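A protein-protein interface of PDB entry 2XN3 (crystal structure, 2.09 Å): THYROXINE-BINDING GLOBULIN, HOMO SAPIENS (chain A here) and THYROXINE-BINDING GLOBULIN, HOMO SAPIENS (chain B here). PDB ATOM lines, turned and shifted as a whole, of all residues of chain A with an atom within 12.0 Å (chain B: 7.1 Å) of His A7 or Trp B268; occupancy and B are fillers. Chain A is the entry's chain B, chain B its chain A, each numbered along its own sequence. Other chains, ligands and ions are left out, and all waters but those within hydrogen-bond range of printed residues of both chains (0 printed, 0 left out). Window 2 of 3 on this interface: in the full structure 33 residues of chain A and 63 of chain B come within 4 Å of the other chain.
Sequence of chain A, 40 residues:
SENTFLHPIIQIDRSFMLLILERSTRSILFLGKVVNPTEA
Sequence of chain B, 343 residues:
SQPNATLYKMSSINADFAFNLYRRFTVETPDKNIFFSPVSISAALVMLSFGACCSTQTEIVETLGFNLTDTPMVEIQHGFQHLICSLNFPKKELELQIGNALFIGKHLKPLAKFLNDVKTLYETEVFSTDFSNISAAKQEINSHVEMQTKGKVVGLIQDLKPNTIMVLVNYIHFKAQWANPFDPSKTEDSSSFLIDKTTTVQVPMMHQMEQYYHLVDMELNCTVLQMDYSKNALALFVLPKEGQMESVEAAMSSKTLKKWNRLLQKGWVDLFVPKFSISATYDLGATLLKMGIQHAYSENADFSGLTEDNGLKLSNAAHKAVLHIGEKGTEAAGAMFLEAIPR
N of Asp B270 lies within hydrogen-bond range of O of Pro A8 (3.0 Å).
The backbone carbonyl oxygen (O) of Asp B270 is in hydrogen-bond range of the backbone NH (N) of Ile A10 (2.9 Å).
The side-chain amide nitrogen of Gln B211 lies close to the indole nitrogen of Trp B268 (3.3 Å).
A ring nitrogen (ND1) of His B214 lies within hydrogen-bond range of the backbone carbonyl oxygen (O) of Tyr B212 (3.1 Å).
The backbone NH (N) of His B214 sits at hydrogen-bond distance from the backbone carbonyl oxygen (O) of Gln B265 (2.9 Å).
The backbone carbonyl oxygen (O) of Glu B210 lies within hydrogen-bond range of the backbone NH (N) of Val B269.
CB of Trp B268 touches ND1 of His A7 (3.6 Å).
His B214 touches Pro A8.
O of Trp B268 touches CD of Pro A8, 3.5 Å away.
Pro A8 touches Val B269.
Ile A9 touches Asp B270 (CA to O, 3.3 Å).
CG1 of Ile A10 touches CG1 of Val B269, at 3.96 Å.
Of the printed residues of chain A, Trp B268 touches His A7 and Pro A8.
No residue of chain A comes within 4 Å of Gln B211.
No residue of chain A comes within 4 Å of Gly B267.
Val B269 touches just these residues of chain A: Pro A8 (3.5 Å) and Ile A10 (3.96 Å).
Of the printed residues of chain A, Asp B270 touches Pro A8 (3.0 Å), Ile A9 (3.3 Å) and Ile A10 (2.9 Å).
Of the printed residues of chain B, Pro A8 touches His B214 (3.995 Å), Trp B268 (3.5 Å), Val B269 (3.5 Å) and Asp B270 (3.0 Å).
Printed residues of chain B within 4 Å of Ile A9: Asp B270.
Of the printed residues of chain B, Ile A10 touches Val B269 (3.96 Å) and Asp B270 (2.9 Å).
Of the printed residues of chain A, His B214 touches Pro A8 (3.995 Å).
The nearest residue of chain B that does not touch His A7 is Val B269 (4.6 Å).
The nearest printed residue of chain A that does not touch His B214 is Ile A10 (4.1 Å).
Printed residues of chain A that touch a printed residue of chain B: His A7, Pro A8, Ile A9 and Ile A10.
Hydrophobic or aromatic side chains of chain A that line the printed part of chain B: His A7, Pro A8, Ile A9 and Ile A10.
Along chain A the printed residues that touch a printed residue of chain B span positions 7 to 10.
Among the printed residues, 8 pairs touch across the chains.
Among the printed residues, no Asp or Glu carboxylate lies within 4 Å of a Lys or Arg side-chain nitrogen of the other chain.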
ATOM      1  N   LEU A   6       3.752  37.311  21.066  1.00  0.00           N
ATOM      2  CA  LEU A   6       3.527  37.576  19.610  1.00  0.00           C
ATOM      3  C   LEU A   6       2.335  36.767  19.064  1.00  0.00           C
ATOM      4  O   LEU A   6       2.057  36.796  17.846  1.00  0.00           O
ATOM      5  CB  LEU A   6       4.807  37.258  18.810  1.00  0.00           C
ATOM      6  N   HIS A   7       1.623  36.062  19.950  1.00  0.00           N
ATOM      7  CA  HIS A   7       0.643  35.073  19.527  1.00  0.00           C
ATOM      8  C   HIS A   7      -0.772  35.641  19.546  1.00  0.00           C
ATOM      9  O   HIS A   7      -1.147  36.330  20.488  1.00  0.00           O
ATOM     10  CB  HIS A   7       0.686  33.840  20.432  1.00  0.00           C
ATOM     11  CG  HIS A   7       2.058  33.272  20.632  1.00  0.00           C
ATOM     12  ND1 HIS A   7       2.984  33.177  19.616  1.00  0.00           N
ATOM     13  CD2 HIS A   7       2.653  32.748  21.729  1.00  0.00           C
ATOM     14  CE1 HIS A   7       4.095  32.632  20.079  1.00  0.00           C
ATOM     15  NE2 HIS A   7       3.919  32.359  21.359  1.00  0.00           N
ATOM     16  N   PRO A   8      -1.572  35.329  18.512  1.00  0.00           N
ATOM     17  CA  PRO A   8      -2.950  35.792  18.503  1.00  0.00           C
ATOM     18  C   PRO A   8      -3.743  35.213  19.671  1.00  0.00           C
ATOM     19  O   PRO A   8      -3.519  34.061  20.084  1.00  0.00           O
ATOM     20  CB  PRO A   8      -3.498  35.267  17.171  1.00  0.00           C
ATOM     21  CG  PRO A   8      -2.570  34.203  16.757  1.00  0.00           C
ATOM     22  CD  PRO A   8      -1.247  34.532  17.319  1.00  0.00           C
ATOM     23  N   ILE A   9      -4.617  36.044  20.222  1.00  0.00           N
ATOM     24  CA  ILE A   9      -5.542  35.631  21.257  1.00  0.00           C
ATOM     25  C   ILE A   9      -6.851  35.306  20.549  1.00  0.00           C
ATOM     26  O   ILE A   9      -7.367  36.140  19.789  1.00  0.00           O
ATOM     27  CB  ILE A   9      -5.764  36.758  22.286  1.00  0.00           C
ATOM     28  CG1 ILE A   9      -4.467  37.065  23.052  1.00  0.00           C
ATOM     29  CG2 ILE A   9      -6.885  36.389  23.258  1.00  0.00           C
ATOM     30  CD1 ILE A   9      -4.402  38.474  23.653  1.00  0.00           C
ATOM     31  N   ILE A  10      -7.377  34.102  20.760  1.00  0.00           N
ATOM     32  CA  ILE A  10      -8.760  33.794  20.350  1.00  0.00           C
ATOM     33  C   ILE A  10      -9.602  33.596  21.585  1.00  0.00           C
ATOM     34  O   ILE A  10      -9.299  32.756  22.437  1.00  0.00           O
ATOM     35  CB  ILE A  10      -8.862  32.587  19.395  1.00  0.00           C
ATOM     36  CG1 ILE A  10      -8.102  32.895  18.075  1.00  0.00           C
ATOM     37  CG2 ILE A  10     -10.326  32.284  19.089  1.00  0.00           C
ATOM     38  CD1 ILE A  10      -8.060  31.721  17.068  1.00  0.00           C
ATOM     39  N   GLN A  11     -10.652  34.401  21.693  1.00  0.00           N
ATOM     40  CA  GLN A  11     -11.530  34.373  22.847  1.00  0.00           C
ATOM     41  C   GLN A  11     -12.934  34.072  22.381  1.00  0.00           C
ATOM     42  O   GLN A  11     -13.579  34.917  21.778  1.00  0.00           O
ATOM     43  CB  GLN A  11     -11.543  35.731  23.555  1.00  0.00           C
ATOM     44  CG  GLN A  11     -10.280  36.065  24.275  1.00  0.00           C
ATOM     45  CD  GLN A  11     -10.345  37.431  24.926  1.00  0.00           C
ATOM     46  OE1 GLN A  11     -10.038  38.431  24.296  1.00  0.00           O
ATOM     47  NE2 GLN A  11     -10.765  37.476  26.185  1.00  0.00           N
ATOM     48  N   MET B 209      -2.758  27.596  26.220  1.00  0.00           N
ATOM     49  CA  MET B 209      -1.814  28.115  25.261  1.00  0.00           C
ATOM     50  C   MET B 209      -1.167  26.921  24.552  1.00  0.00           C
ATOM     51  O   MET B 209      -0.388  26.182  25.146  1.00  0.00           O
ATOM     52  CB  MET B 209      -0.749  28.939  25.973  1.00  0.00           C
ATOM     53  CG  MET B 209      -1.256  30.010  26.928  1.00  0.00           C
ATOM     54  SD  MET B 209       0.135  30.895  27.675  1.00  0.00           S
ATOM     55  CE  MET B 209      -0.773  32.035  28.719  1.00  0.00           C
ATOM     56  N   GLU B 210      -1.531  26.716  23.294  1.00  0.00           N
ATOM     57  CA  GLU B 210      -1.066  25.583  22.498  1.00  0.00           C
ATOM     58  C   GLU B 210      -1.100  26.008  21.013  1.00  0.00           C
ATOM     59  O   GLU B 210      -1.573  27.109  20.677  1.00  0.00           O
ATOM     60  CB  GLU B 210      -1.940  24.313  22.746  1.00  0.00           C
ATOM     61  CG  GLU B 210      -1.289  23.223  23.681  1.00  0.00           C
ATOM     62  CD  GLU B 210      -0.020  22.627  23.098  1.00  0.00           C
ATOM     63  OE1 GLU B 210       0.108  22.696  21.852  1.00  0.00           O
ATOM     64  OE2 GLU B 210       0.862  22.104  23.863  1.00  0.00           O
ATOM     65  N   GLN B 211      -0.608  25.131  20.149  1.00  0.00           N
ATOM     66  CA  GLN B 211      -0.734  25.306  18.713  1.00  0.00           C
ATOM     67  C   GLN B 211      -2.056  24.740  18.224  1.00  0.00           C
ATOM     68  O   GLN B 211      -2.378  23.613  18.549  1.00  0.00           O
ATOM     69  CB  GLN B 211       0.382  24.586  17.986  1.00  0.00           C
ATOM     70  CG  GLN B 211       1.732  25.179  18.188  1.00  0.00           C
ATOM     71  CD  GLN B 211       2.765  24.573  17.244  1.00  0.00           C
ATOM     72  OE1 GLN B 211       2.523  23.546  16.620  1.00  0.00           O
ATOM     73  NE2 GLN B 211       3.919  25.206  17.144  1.00  0.00           N
ATOM     74  N   TYR B 212      -2.801  25.521  17.436  1.00  0.00           N
ATOM     75  CA  TYR B 212      -4.040  25.062  16.822  1.00  0.00           C
ATOM     76  C   TYR B 212      -4.081  25.464  15.347  1.00  0.00           C
ATOM     77  O   TYR B 212      -3.493  26.480  14.932  1.00  0.00           O
ATOM     78  CB  TYR B 212      -5.266  25.667  17.526  1.00  0.00           C
ATOM     79  CG  TYR B 212      -5.457  25.238  18.982  1.00  0.00           C
ATOM     80  CD1 TYR B 212      -6.091  24.062  19.301  1.00  0.00           C
ATOM     81  CD2 TYR B 212      -4.990  26.022  20.025  1.00  0.00           C
ATOM     82  CE1 TYR B 212      -6.265  23.666  20.635  1.00  0.00           C
ATOM     83  CE2 TYR B 212      -5.156  25.637  21.375  1.00  0.00           C
ATOM     84  CZ  TYR B 212      -5.788  24.461  21.662  1.00  0.00           C
ATOM     85  OH  TYR B 212      -5.970  24.086  22.970  1.00  0.00           O
ATOM     86  N   HIS B 214      -5.920  27.279  12.775  1.00  0.00           N
ATOM     87  CA  HIS B 214      -6.896  28.368  12.827  1.00  0.00           C
ATOM     88  C   HIS B 214      -6.718  29.249  11.616  1.00  0.00           C
ATOM     89  O   HIS B 214      -5.729  29.115  10.880  1.00  0.00           O
ATOM     90  CB  HIS B 214      -6.717  29.180  14.103  1.00  0.00           C
ATOM     91  CG  HIS B 214      -5.456  29.993  14.135  1.00  0.00           C
ATOM     92  ND1 HIS B 214      -4.209  29.433  14.355  1.00  0.00           N
ATOM     93  CD2 HIS B 214      -5.252  31.321  13.980  1.00  0.00           C
ATOM     94  CE1 HIS B 214      -3.296  30.389  14.331  1.00  0.00           C
ATOM     95  NE2 HIS B 214      -3.901  31.543  14.090  1.00  0.00           N
ATOM     96  N   GLN B 265      -4.249  27.047   9.138  1.00  0.00           N
ATOM     97  CA  GLN B 265      -2.830  26.840   9.443  1.00  0.00           C
ATOM     98  C   GLN B 265      -2.620  26.659  10.942  1.00  0.00           C
ATOM     99  O   GLN B 265      -3.238  27.327  11.776  1.00  0.00           O
ATOM    100  CB  GLN B 265      -1.963  27.990   8.926  1.00  0.00           C
ATOM    101  CG  GLN B 265      -0.467  27.668   9.114  1.00  0.00           C
ATOM    102  CD  GLN B 265       0.474  28.696   8.581  1.00  0.00           C
ATOM    103  OE1 GLN B 265       1.702  28.479   8.599  1.00  0.00           O
ATOM    104  NE2 GLN B 265      -0.068  29.836   8.108  1.00  0.00           N
ATOM    105  N   LYS B 266      -1.719  25.747  11.272  1.00  0.00           N
ATOM    106  CA  LYS B 266      -1.362  25.495  12.648  1.00  0.00           C
ATOM    107  C   LYS B 266      -0.410  26.576  13.125  1.00  0.00           C
ATOM    108  O   LYS B 266       0.559  26.922  12.441  1.00  0.00           O
ATOM    109  CB  LYS B 266      -0.730  24.101  12.818  1.00  0.00           C
ATOM    110  CG  LYS B 266      -0.697  23.624  14.264  1.00  0.00           C
ATOM    111  CD  LYS B 266      -0.276  22.152  14.390  1.00  0.00           C
ATOM    112  CE  LYS B 266      -1.041  21.484  15.527  1.00  0.00           C
ATOM    113  NZ  LYS B 266      -0.935  19.984  15.513  1.00  0.00           N
ATOM    114  N   GLY B 267      -0.699  27.121  14.294  1.00  0.00           N
ATOM    115  CA  GLY B 267       0.213  28.045  14.951  1.00  0.00           C
ATOM    116  C   GLY B 267      -0.204  28.291  16.383  1.00  0.00           C
ATOM    117  O   GLY B 267      -1.297  27.856  16.807  1.00  0.00           O
ATOM    118  N   TRP B 268       0.646  29.002  17.123  1.00  0.00           N
ATOM    119  CA  TRP B 268       0.391  29.252  18.540  1.00  0.00           C
ATOM    120  C   TRP B 268      -0.804  30.178  18.733  1.00  0.00           C
ATOM    121  O   TRP B 268      -1.003  31.127  17.983  1.00  0.00           O
ATOM    122  CB  TRP B 268       1.612  29.840  19.228  1.00  0.00           C
ATOM    123  CG  TRP B 268       2.734  28.895  19.321  1.00  0.00           C
ATOM    124  CD1 TRP B 268       3.856  28.864  18.538  1.00  0.00           C
ATOM    125  CD2 TRP B 268       2.856  27.814  20.251  1.00  0.00           C
ATOM    126  NE1 TRP B 268       4.665  27.825  18.926  1.00  0.00           N
ATOM    127  CE2 TRP B 268       4.083  27.172  19.985  1.00  0.00           C
ATOM    128  CE3 TRP B 268       2.053  27.340  21.302  1.00  0.00           C
ATOM    129  CZ2 TRP B 268       4.524  26.064  20.718  1.00  0.00           C
ATOM    130  CZ3 TRP B 268       2.501  26.235  22.045  1.00  0.00           C
ATOM    131  CH2 TRP B 268       3.715  25.610  21.738  1.00  0.00           C
ATOM    132  N   VAL B 269      -1.600  29.878  19.743  1.00  0.00           N
ATOM    133  CA  VAL B 269      -2.797  30.655  20.052  1.00  0.00           C
ATOM    134  C   VAL B 269      -2.966  30.693  21.550  1.00  0.00           C
ATOM    135  O   VAL B 269      -2.717  29.681  22.234  1.00  0.00           O
ATOM    136  CB  VAL B 269      -4.055  30.019  19.449  1.00  0.00           C
ATOM    137  CG1 VAL B 269      -5.310  30.756  19.905  1.00  0.00           C
ATOM    138  CG2 VAL B 269      -3.972  29.989  17.926  1.00  0.00           C
ATOM    139  N   ASP B 270      -3.355  31.867  22.059  1.00  0.00           N
ATOM    140  CA  ASP B 270      -3.770  32.011  23.439  1.00  0.00           C
ATOM    141  C   ASP B 270      -5.276  31.904  23.398  1.00  0.00           C
ATOM    142  O   ASP B 270      -5.954  32.818  22.927  1.00  0.00           O
ATOM    143  CB  ASP B 270      -3.284  33.359  23.997  1.00  0.00           C
ATOM    144  CG  ASP B 270      -3.454  33.481  25.505  1.00  0.00           C
ATOM    145  OD1 ASP B 270      -3.648  32.455  26.214  1.00  0.00           O
ATOM    146  OD2 ASP B 270      -3.388  34.625  25.993  1.00  0.00           O
